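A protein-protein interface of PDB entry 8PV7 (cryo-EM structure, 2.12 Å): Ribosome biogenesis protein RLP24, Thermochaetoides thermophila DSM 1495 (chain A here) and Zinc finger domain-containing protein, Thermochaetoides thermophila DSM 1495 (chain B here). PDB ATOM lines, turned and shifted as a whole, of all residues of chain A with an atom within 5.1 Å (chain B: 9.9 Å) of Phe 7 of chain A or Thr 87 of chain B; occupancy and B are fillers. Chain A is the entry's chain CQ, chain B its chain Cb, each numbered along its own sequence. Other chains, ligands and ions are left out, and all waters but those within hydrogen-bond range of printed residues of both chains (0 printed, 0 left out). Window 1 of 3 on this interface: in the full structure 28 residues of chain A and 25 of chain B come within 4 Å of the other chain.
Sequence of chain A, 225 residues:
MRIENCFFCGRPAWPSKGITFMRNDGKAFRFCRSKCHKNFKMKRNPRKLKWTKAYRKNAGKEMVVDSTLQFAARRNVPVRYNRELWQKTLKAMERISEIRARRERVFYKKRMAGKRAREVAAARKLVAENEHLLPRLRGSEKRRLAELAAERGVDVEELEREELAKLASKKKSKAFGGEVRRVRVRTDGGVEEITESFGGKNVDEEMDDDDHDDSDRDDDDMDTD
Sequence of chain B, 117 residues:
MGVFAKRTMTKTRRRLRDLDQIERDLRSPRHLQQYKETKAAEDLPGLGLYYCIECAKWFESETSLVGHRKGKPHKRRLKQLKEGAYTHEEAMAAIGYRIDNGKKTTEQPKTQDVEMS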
ATOM      1  N   ASN A   5      18.459  -2.165 -26.096  1.00  0.00           N
ATOM      2  CA  ASN A   5      18.433  -1.308 -24.927  1.00  0.00           C
ATOM      3  C   ASN A   5      17.094  -0.599 -24.877  1.00  0.00           C
ATOM      4  O   ASN A   5      16.486  -0.318 -25.911  1.00  0.00           O
ATOM      5  CB  ASN A   5      19.588  -0.310 -24.937  1.00  0.00           C
ATOM      6  CG  ASN A   5      20.899  -0.944 -24.518  1.00  0.00           C
ATOM      7  OD1 ASN A   5      21.287  -0.885 -23.354  1.00  0.00           O
ATOM      8  ND2 ASN A   5      21.580  -1.569 -25.465  1.00  0.00           N
ATOM      9  N   CYS A   6      16.623  -0.350 -23.661  1.00  0.00           N
ATOM     10  CA  CYS A   6      15.345   0.319 -23.486  1.00  0.00           C
ATOM     11  C   CYS A   6      15.448   1.760 -23.964  1.00  0.00           C
ATOM     12  O   CYS A   6      16.432   2.450 -23.692  1.00  0.00           O
ATOM     13  CB  CYS A   6      14.909   0.275 -22.023  1.00  0.00           C
ATOM     14  SG  CYS A   6      13.332   1.089 -21.695  1.00  0.00           S
ATOM     15  N   PHE A   7      14.436   2.198 -24.710  1.00  0.00           N
ATOM     16  CA  PHE A   7      14.392   3.580 -25.170  1.00  0.00           C
ATOM     17  C   PHE A   7      14.279   4.541 -23.996  1.00  0.00           C
ATOM     18  O   PHE A   7      14.938   5.584 -23.973  1.00  0.00           O
ATOM     19  CB  PHE A   7      13.223   3.764 -26.141  1.00  0.00           C
ATOM     20  CG  PHE A   7      12.956   5.195 -26.517  1.00  0.00           C
ATOM     21  CD1 PHE A   7      13.759   5.844 -27.436  1.00  0.00           C
ATOM     22  CD2 PHE A   7      11.892   5.886 -25.959  1.00  0.00           C
ATOM     23  CE1 PHE A   7      13.516   7.151 -27.779  1.00  0.00           C
ATOM     24  CE2 PHE A   7      11.649   7.198 -26.298  1.00  0.00           C
ATOM     25  CZ  PHE A   7      12.458   7.829 -27.211  1.00  0.00           C
ATOM     26  N   PHE A   8      13.476   4.187 -22.998  1.00  0.00           N
ATOM     27  CA  PHE A   8      13.174   5.112 -21.915  1.00  0.00           C
ATOM     28  C   PHE A   8      14.281   5.150 -20.868  1.00  0.00           C
ATOM     29  O   PHE A   8      14.752   6.227 -20.500  1.00  0.00           O
ATOM     30  CB  PHE A   8      11.838   4.738 -21.276  1.00  0.00           C
ATOM     31  CG  PHE A   8      11.160   5.879 -20.586  1.00  0.00           C
ATOM     32  CD1 PHE A   8      11.452   6.177 -19.267  1.00  0.00           C
ATOM     33  CD2 PHE A   8      10.230   6.653 -21.255  1.00  0.00           C
ATOM     34  CE1 PHE A   8      10.832   7.226 -18.632  1.00  0.00           C
ATOM     35  CE2 PHE A   8       9.603   7.699 -20.622  1.00  0.00           C
ATOM     36  CZ  PHE A   8       9.906   7.988 -19.311  1.00  0.00           C
ATOM     37  N   CYS A   9      14.706   3.991 -20.370  1.00  0.00           N
ATOM     38  CA  CYS A   9      15.617   3.949 -19.236  1.00  0.00           C
ATOM     39  C   CYS A   9      17.009   3.425 -19.565  1.00  0.00           C
ATOM     40  O   CYS A   9      17.902   3.544 -18.724  1.00  0.00           O
ATOM     41  CB  CYS A   9      15.018   3.102 -18.108  1.00  0.00           C
ATOM     42  SG  CYS A   9      15.148   1.334 -18.366  1.00  0.00           S
ATOM     43  N   GLY A  10      17.216   2.834 -20.738  1.00  0.00           N
ATOM     44  CA  GLY A  10      18.530   2.393 -21.148  1.00  0.00           C
ATOM     45  C   GLY A  10      18.980   1.049 -20.611  1.00  0.00           C
ATOM     46  O   GLY A  10      20.126   0.661 -20.860  1.00  0.00           O
ATOM     47  N   PHE A  29       9.754   1.994 -30.891  1.00  0.00           N
ATOM     48  CA  PHE A  29      10.163   2.331 -29.532  1.00  0.00           C
ATOM     49  C   PHE A  29      10.139   1.061 -28.696  1.00  0.00           C
ATOM     50  O   PHE A  29       9.066   0.528 -28.407  1.00  0.00           O
ATOM     51  CB  PHE A  29       9.245   3.391 -28.926  1.00  0.00           C
ATOM     52  CG  PHE A  29       9.279   4.702 -29.642  1.00  0.00           C
ATOM     53  CD1 PHE A  29       8.458   4.936 -30.734  1.00  0.00           C
ATOM     54  CD2 PHE A  29      10.134   5.706 -29.225  1.00  0.00           C
ATOM     55  CE1 PHE A  29       8.491   6.147 -31.393  1.00  0.00           C
ATOM     56  CE2 PHE A  29      10.170   6.914 -29.878  1.00  0.00           C
ATOM     57  CZ  PHE A  29       9.349   7.135 -30.965  1.00  0.00           C
ATOM     58  N   ARG A  30      11.309   0.585 -28.291  1.00  0.00           N
ATOM     59  CA  ARG A  30      11.404  -0.624 -27.489  1.00  0.00           C
ATOM     60  C   ARG A  30      11.512  -0.267 -26.012  1.00  0.00           C
ATOM     61  O   ARG A  30      12.381   0.514 -25.618  1.00  0.00           O
ATOM     62  CB  ARG A  30      12.608  -1.458 -27.924  1.00  0.00           C
ATOM     63  CG  ARG A  30      12.902  -2.626 -27.012  1.00  0.00           C
ATOM     64  CD  ARG A  30      11.838  -3.703 -27.126  1.00  0.00           C
ATOM     65  NE  ARG A  30      12.080  -4.807 -26.206  1.00  0.00           N
ATOM     66  CZ  ARG A  30      12.905  -5.815 -26.446  1.00  0.00           C
ATOM     67  NH1 ARG A  30      13.565  -5.910 -27.585  1.00  0.00           N
ATOM     68  NH2 ARG A  30      13.076  -6.750 -25.518  1.00  0.00           N
ATOM     69  N   PHE A  31      10.639  -0.849 -25.197  1.00  0.00           N
ATOM     70  CA  PHE A  31      10.652  -0.668 -23.756  1.00  0.00           C
ATOM     71  C   PHE A  31      10.940  -1.995 -23.082  1.00  0.00           C
ATOM     72  O   PHE A  31      10.424  -3.039 -23.488  1.00  0.00           O
ATOM     73  CB  PHE A  31       9.320  -0.108 -23.250  1.00  0.00           C
ATOM     74  CG  PHE A  31       8.896   1.130 -23.957  1.00  0.00           C
ATOM     75  CD1 PHE A  31       9.470   2.344 -23.643  1.00  0.00           C
ATOM     76  CD2 PHE A  31       7.946   1.081 -24.959  1.00  0.00           C
ATOM     77  CE1 PHE A  31       9.099   3.482 -24.304  1.00  0.00           C
ATOM     78  CE2 PHE A  31       7.573   2.218 -25.622  1.00  0.00           C
ATOM     79  CZ  PHE A  31       8.154   3.416 -25.296  1.00  0.00           C
ATOM     80  N   PHE A  40       6.171   6.439 -20.673  1.00  0.00           N
ATOM     81  CA  PHE A  40       6.155   6.955 -22.038  1.00  0.00           C
ATOM     82  C   PHE A  40       4.743   7.330 -22.484  1.00  0.00           C
ATOM     83  O   PHE A  40       4.543   8.387 -23.090  1.00  0.00           O
ATOM     84  CB  PHE A  40       6.761   5.916 -22.980  1.00  0.00           C
ATOM     85  CG  PHE A  40       6.785   6.328 -24.424  1.00  0.00           C
ATOM     86  CD1 PHE A  40       7.831   7.079 -24.921  1.00  0.00           C
ATOM     87  CD2 PHE A  40       5.780   5.927 -25.293  1.00  0.00           C
ATOM     88  CE1 PHE A  40       7.864   7.445 -26.245  1.00  0.00           C
ATOM     89  CE2 PHE A  40       5.808   6.294 -26.615  1.00  0.00           C
ATOM     90  CZ  PHE A  40       6.853   7.052 -27.093  1.00  0.00           C
ATOM     91  N   ASP B  18       3.278  13.506 -30.376  1.00  0.00           N
ATOM     92  CA  ASP B  18       4.454  13.496 -29.516  1.00  0.00           C
ATOM     93  C   ASP B  18       5.333  14.723 -29.737  1.00  0.00           C
ATOM     94  O   ASP B  18       5.288  15.378 -30.785  1.00  0.00           O
ATOM     95  CB  ASP B  18       5.275  12.230 -29.754  1.00  0.00           C
ATOM     96  CG  ASP B  18       5.067  11.191 -28.675  1.00  0.00           C
ATOM     97  OD1 ASP B  18       5.227  11.530 -27.484  1.00  0.00           O
ATOM     98  OD2 ASP B  18       4.750  10.033 -29.017  1.00  0.00           O
ATOM     99  N   LEU B  19       6.165  15.008 -28.730  1.00  0.00           N
ATOM    100  CA  LEU B  19       6.965  16.229 -28.726  1.00  0.00           C
ATOM    101  C   LEU B  19       8.046  16.209 -29.801  1.00  0.00           C
ATOM    102  O   LEU B  19       8.355  17.249 -30.389  1.00  0.00           O
ATOM    103  CB  LEU B  19       7.592  16.440 -27.350  1.00  0.00           C
ATOM    104  CG  LEU B  19       8.084  17.860 -27.075  1.00  0.00           C
ATOM    105  CD1 LEU B  19       6.925  18.838 -27.061  1.00  0.00           C
ATOM    106  CD2 LEU B  19       8.854  17.920 -25.774  1.00  0.00           C
ATOM    107  N   ASP B  20       8.648  15.047 -30.063  1.00  0.00           N
ATOM    108  CA  ASP B  20       9.653  14.977 -31.120  1.00  0.00           C
ATOM    109  C   ASP B  20       9.018  15.142 -32.495  1.00  0.00           C
ATOM    110  O   ASP B  20       9.624  15.729 -33.401  1.00  0.00           O
ATOM    111  CB  ASP B  20      10.434  13.666 -31.031  1.00  0.00           C
ATOM    112  CG  ASP B  20       9.538  12.448 -31.049  1.00  0.00           C
ATOM    113  OD1 ASP B  20       9.844  11.495 -31.793  1.00  0.00           O
ATOM    114  OD2 ASP B  20       8.535  12.439 -30.310  1.00  0.00           O
ATOM    115  N   GLN B  21       7.790  14.646 -32.662  1.00  0.00           N
ATOM    116  CA  GLN B  21       7.053  14.900 -33.894  1.00  0.00           C
ATOM    117  C   GLN B  21       6.743  16.381 -34.051  1.00  0.00           C
ATOM    118  O   GLN B  21       6.810  16.919 -35.159  1.00  0.00           O
ATOM    119  CB  GLN B  21       5.765  14.081 -33.919  1.00  0.00           C
ATOM    120  CG  GLN B  21       5.980  12.595 -33.738  1.00  0.00           C
ATOM    121  CD  GLN B  21       4.685  11.818 -33.723  1.00  0.00           C
ATOM    122  OE1 GLN B  21       3.916  11.887 -32.768  1.00  0.00           O
ATOM    123  NE2 GLN B  21       4.434  11.072 -34.789  1.00  0.00           N
ATOM    124  N   ILE B  22       6.421  17.056 -32.948  1.00  0.00           N
ATOM    125  CA  ILE B  22       6.168  18.494 -32.993  1.00  0.00           C
ATOM    126  C   ILE B  22       7.452  19.257 -33.323  1.00  0.00           C
ATOM    127  O   ILE B  22       7.431  20.252 -34.059  1.00  0.00           O
ATOM    128  CB  ILE B  22       5.528  18.940 -31.663  1.00  0.00           C
ATOM    129  CG1 ILE B  22       4.102  18.393 -31.580  1.00  0.00           C
ATOM    130  CG2 ILE B  22       5.525  20.450 -31.506  1.00  0.00           C
ATOM    131  CD1 ILE B  22       3.503  18.422 -30.210  1.00  0.00           C
ATOM    132  N   GLU B  23       8.588  18.785 -32.806  1.00  0.00           N
ATOM    133  CA  GLU B  23       9.883  19.379 -33.140  1.00  0.00           C
ATOM    134  C   GLU B  23      10.190  19.246 -34.626  1.00  0.00           C
ATOM    135  O   GLU B  23      10.645  20.201 -35.271  1.00  0.00           O
ATOM    136  CB  GLU B  23      10.987  18.719 -32.315  1.00  0.00           C
ATOM    137  CG  GLU B  23      11.622  19.618 -31.287  1.00  0.00           C
ATOM    138  CD  GLU B  23      12.756  18.945 -30.546  1.00  0.00           C
ATOM    139  OE1 GLU B  23      13.295  19.556 -29.601  1.00  0.00           O
ATOM    140  OE2 GLU B  23      13.118  17.811 -30.914  1.00  0.00           O
ATOM    141  N   ARG B  24       9.943  18.061 -35.188  1.00  0.00           N
ATOM    142  CA  ARG B  24      10.146  17.864 -36.620  1.00  0.00           C
ATOM    143  C   ARG B  24       9.161  18.691 -37.440  1.00  0.00           C
ATOM    144  O   ARG B  24       9.488  19.142 -38.541  1.00  0.00           O
ATOM    145  CB  ARG B  24      10.027  16.382 -36.966  1.00  0.00           C
ATOM    146  CG  ARG B  24      11.350  15.710 -37.259  1.00  0.00           C
ATOM    147  CD  ARG B  24      11.214  14.200 -37.288  1.00  0.00           C
ATOM    148  NE  ARG B  24      11.436  13.611 -35.972  1.00  0.00           N
ATOM    149  CZ  ARG B  24      10.625  12.734 -35.395  1.00  0.00           C
ATOM    150  NH1 ARG B  24       9.525  12.311 -35.996  1.00  0.00           N
ATOM    151  NH2 ARG B  24      10.925  12.272 -34.184  1.00  0.00           N
ATOM    152  N   ARG B  27      10.626  22.190 -37.473  1.00  0.00           N
ATOM    153  CA  ARG B  27      11.808  22.291 -38.323  1.00  0.00           C
ATOM    154  C   ARG B  27      11.467  22.182 -39.805  1.00  0.00           C
ATOM    155  O   ARG B  27      12.019  22.927 -40.622  1.00  0.00           O
ATOM    156  CB  ARG B  27      12.821  21.216 -37.935  1.00  0.00           C
ATOM    157  CG  ARG B  27      13.926  21.711 -37.028  1.00  0.00           C
ATOM    158  CD  ARG B  27      14.857  20.583 -36.618  1.00  0.00           C
ATOM    159  NE  ARG B  27      14.752  19.426 -37.496  1.00  0.00           N
ATOM    160  CZ  ARG B  27      14.407  18.210 -37.092  1.00  0.00           C
ATOM    161  NH1 ARG B  27      14.131  17.957 -35.823  1.00  0.00           N
ATOM    162  NH2 ARG B  27      14.334  17.226 -37.984  1.00  0.00           N
ATOM    163  N   GLU B  83      13.769  23.038 -23.894  1.00  0.00           N
ATOM    164  CA  GLU B  83      14.612  22.016 -23.286  1.00  0.00           C
ATOM    165  C   GLU B  83      15.009  20.944 -24.293  1.00  0.00           C
ATOM    166  O   GLU B  83      16.101  20.376 -24.192  1.00  0.00           O
ATOM    167  CB  GLU B  83      13.895  21.384 -22.096  1.00  0.00           C
ATOM    168  CG  GLU B  83      14.015  22.178 -20.814  1.00  0.00           C
ATOM    169  CD  GLU B  83      13.451  21.440 -19.621  1.00  0.00           C
ATOM    170  OE1 GLU B  83      13.765  20.242 -19.462  1.00  0.00           O
ATOM    171  OE2 GLU B  83      12.695  22.056 -18.843  1.00  0.00           O
ATOM    172  N   GLY B  84      14.151  20.659 -25.266  1.00  0.00           N
ATOM    173  CA  GLY B  84      14.481  19.690 -26.290  1.00  0.00           C
ATOM    174  C   GLY B  84      13.800  18.356 -26.085  1.00  0.00           C
ATOM    175  O   GLY B  84      13.795  17.816 -24.978  1.00  0.00           O
ATOM    176  N   ALA B  85      13.217  17.816 -27.149  1.00  0.00           N
ATOM    177  CA  ALA B  85      12.519  16.545 -27.060  1.00  0.00           C
ATOM    178  C   ALA B  85      13.502  15.385 -26.957  1.00  0.00           C
ATOM    179  O   ALA B  85      14.618  15.435 -27.479  1.00  0.00           O
ATOM    180  CB  ALA B  85      11.608  16.354 -28.268  1.00  0.00           C
ATOM    181  N   TYR B  86      13.073  14.333 -26.272  1.00  0.00           N
ATOM    182  CA  TYR B  86      13.874  13.127 -26.138  1.00  0.00           C
ATOM    183  C   TYR B  86      13.765  12.276 -27.397  1.00  0.00           C
ATOM    184  O   TYR B  86      12.666  11.999 -27.881  1.00  0.00           O
ATOM    185  CB  TYR B  86      13.415  12.333 -24.919  1.00  0.00           C
ATOM    186  CG  TYR B  86      14.313  11.189 -24.531  1.00  0.00           C
ATOM    187  CD1 TYR B  86      15.575  11.418 -24.008  1.00  0.00           C
ATOM    188  CD2 TYR B  86      13.893   9.877 -24.677  1.00  0.00           C
ATOM    189  CE1 TYR B  86      16.394  10.376 -23.652  1.00  0.00           C
ATOM    190  CE2 TYR B  86      14.704   8.829 -24.319  1.00  0.00           C
ATOM    191  CZ  TYR B  86      15.952   9.083 -23.807  1.00  0.00           C
ATOM    192  OH  TYR B  86      16.758   8.038 -23.445  1.00  0.00           O
ATOM    193  N   THR B  87      14.911  11.866 -27.930  1.00  0.00           N
ATOM    194  CA  THR B  87      14.976  11.152 -29.198  1.00  0.00           C
ATOM    195  C   THR B  87      15.801   9.880 -29.041  1.00  0.00           C
ATOM    196  O   THR B  87      16.399   9.616 -27.992  1.00  0.00           O
ATOM    197  CB  THR B  87      15.575  12.030 -30.308  1.00  0.00           C
ATOM    198  OG1 THR B  87      16.853  12.524 -29.894  1.00  0.00           O
ATOM    199  CG2 THR B  87      14.663  13.197 -30.632  1.00  0.00           C
ATOM    200  N   HIS B  88      15.835   9.094 -30.121  1.00  0.00           N
ATOM    201  CA  HIS B  88      16.655   7.889 -30.153  1.00  0.00           C
ATOM    202  C   HIS B  88      18.140   8.218 -30.125  1.00  0.00           C
ATOM    203  O   HIS B  88      18.932   7.436 -29.592  1.00  0.00           O
ATOM    204  CB  HIS B  88      16.326   7.060 -31.392  1.00  0.00           C
ATOM    205  CG  HIS B  88      15.171   6.130 -31.208  1.00  0.00           C
ATOM    206  ND1 HIS B  88      13.872   6.492 -31.490  1.00  0.00           N
ATOM    207  CD2 HIS B  88      15.117   4.851 -30.768  1.00  0.00           C
ATOM    208  CE1 HIS B  88      13.070   5.476 -31.235  1.00  0.00           C
ATOM    209  NE2 HIS B  88      13.800   4.468 -30.795  1.00  0.00           N
ATOM    210  N   GLU B  89      18.531   9.363 -30.688  1.00  0.00           N
ATOM    211  CA  GLU B  89      19.923   9.796 -30.614  1.00  0.00           C
ATOM    212  C   GLU B  89      20.334  10.088 -29.176  1.00  0.00           C
ATOM    213  O   GLU B  89      21.418   9.680 -28.740  1.00  0.00           O
ATOM    214  CB  GLU B  89      20.157  11.028 -31.498  1.00  0.00           C
ATOM    215  CG  GLU B  89      19.660  10.948 -32.953  1.00  0.00           C
ATOM    216  CD  GLU B  89      18.160  11.172 -33.119  1.00  0.00           C
ATOM    217  OE1 GLU B  89      17.370  10.295 -32.711  1.00  0.00           O
ATOM    218  OE2 GLU B  89      17.772  12.230 -33.660  1.00  0.00           O
ATOM    219  N   GLU B  90      19.472  10.773 -28.420  1.00  0.00           N
ATOM    220  CA  GLU B  90      19.757  11.029 -27.012  1.00  0.00           C
ATOM    221  C   GLU B  90      19.754   9.736 -26.210  1.00  0.00           C
ATOM    222  O   GLU B  90      20.570   9.564 -25.298  1.00  0.00           O
ATOM    223  CB  GLU B  90      18.746  12.022 -26.440  1.00  0.00           C
ATOM    224  CG  GLU B  90      19.029  12.440 -25.006  1.00  0.00           C
ATOM    225  CD  GLU B  90      18.130  13.558 -24.526  1.00  0.00           C
ATOM    226  OE1 GLU B  90      17.367  14.105 -25.348  1.00  0.00           O
ATOM    227  OE2 GLU B  90      18.178  13.887 -23.323  1.00  0.00           O
ATOM    228  N   ALA B  91      18.858   8.806 -26.555  1.00  0.00           N
ATOM    229  CA  ALA B  91      18.835   7.507 -25.890  1.00  0.00           C
ATOM    230  C   ALA B  91      20.121   6.725 -26.132  1.00  0.00           C
ATOM    231  O   ALA B  91      20.644   6.078 -25.218  1.00  0.00           O
ATOM    232  CB  ALA B  91      17.621   6.705 -26.354  1.00  0.00           C
ATOM    233  N   MET B  92      20.639   6.763 -27.360  1.00  0.00           N
ATOM    234  CA  MET B  92      21.896   6.087 -27.665  1.00  0.00           C
ATOM    235  C   MET B  92      23.071   6.747 -26.953  1.00  0.00           C
ATOM    236  O   MET B  92      23.963   6.062 -26.430  1.00  0.00           O
ATOM    237  CB  MET B  92      22.118   6.080 -29.173  1.00  0.00           C
ATOM    238  CG  MET B  92      22.508   4.739 -29.740  1.00  0.00           C
ATOM    239  SD  MET B  92      23.066   4.846 -31.449  1.00  0.00           S
ATOM    240  CE  MET B  92      21.976   6.113 -32.088  1.00  0.00           C
ATOM    241  N   ALA B  93      23.086   8.081 -26.917  1.00  0.00           N
ATOM    242  CA  ALA B  93      24.172   8.787 -26.247  1.00  0.00           C
ATOM    243  C   ALA B  93      24.134   8.585 -24.738  1.00  0.00           C
ATOM    244  O   ALA B  93      25.173   8.685 -24.077  1.00  0.00           O
ATOM    245  CB  ALA B  93      24.115  10.274 -26.587  1.00  0.00           C
ATOM    246  N   ALA B  94      22.953   8.298 -24.182  1.00  0.00           N
ATOM    247  CA  ALA B  94      22.838   8.080 -22.744  1.00  0.00           C
ATOM    248  C   ALA B  94      23.572   6.823 -22.297  1.00  0.00           C
ATOM    249  O   ALA B  94      24.077   6.769 -21.170  1.00  0.00           O
ATOM    250  CB  ALA B  94      21.367   8.004 -22.342  1.00  0.00           C
ATOM    251  N   ILE B  95      23.633   5.803 -23.147  1.00  0.00           N
ATOM    252  CA  ILE B  95      24.370   4.585 -22.849  1.00  0.00           C
ATOM    253  C   ILE B  95      25.721   4.562 -23.545  1.00  0.00           C
ATOM    254  O   ILE B  95      26.477   3.600 -23.385  1.00  0.00           O
ATOM    255  CB  ILE B  95      23.557   3.333 -23.205  1.00  0.00           C
ATOM    256  CG1 ILE B  95      23.196   3.349 -24.687  1.00  0.00           C
ATOM    257  CG2 ILE B  95      22.317   3.245 -22.336  1.00  0.00           C
ATOM    258  CD1 ILE B  95      22.482   2.124 -25.152  1.00  0.00           C
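Of chain B, only Tyr 86, Thr 87, His 88 and Ala 91 come within 4 Å of Phe 7 of chain A. Of the printed residues of chain B, Phe 8 of chain A touches Tyr 86. Cys 9 of chain A touches none of the printed residues of chain B. Of chain A, only Phe 7 comes within 4 Å of Thr 87 of chain B. Printed residues of chain A within 4 Å of Ala 91 of chain B: Phe 7. The nearest printed residue of chain A that does not touch Thr 87 of chain B is Phe 29 of chain A (6.4 Å). The nearest printed residue of chain B that does not touch Asn 5 of chain A is Ala 91 of chain B (6.5 Å).
OH of Tyr 86 of chain B lies within hydrogen-bond range of O of Phe 7 of chain A (3.1 Å).
Hydrophobic or aromatic side chains of chain B within 4 Å of the printed part of chain A: Tyr 86, His 88, Ala 91 and Ile 95. Hydrophobic or aromatic side chains of chain A within 4 Å of the printed part of chain B: Phe 7 and Phe 29. Among the printed residues, 8 pairs touch across the chains.
The side-chain amide oxygen (OD1) of Asn 5 of chain A lies close to the backbone carbonyl oxygen (O) of Gly 10 of chain A, at 3.2 Å. The backbone NH (N) of Phe 8 of chain A lies close to the side-chain sulfur (SG) of Cys 6 of chain A (3.4 Å). O of Arg 30 of chain A is in hydrogen-bond range of N of Phe 7 of chain A (2.8 Å). OG1 of Thr 87 of chain B sits at hydrogen-bond distance from N of Glu 90 of chain B.
Among the printed residues, merely in contact across the chains: Asn 5 of chain A with Ile 95 of chain B, Phe 7 of chain A with Thr 87 of chain B, Phe 7 of chain A with His 88 of chain B, Phe 7 of chain A with Ala 91 of chain B, Phe 8 of chain A with Tyr 86 of chain B, Gly 10 of chain A with Ile 95 of chain B and Phe 29 of chain A with His 88 of chain B.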
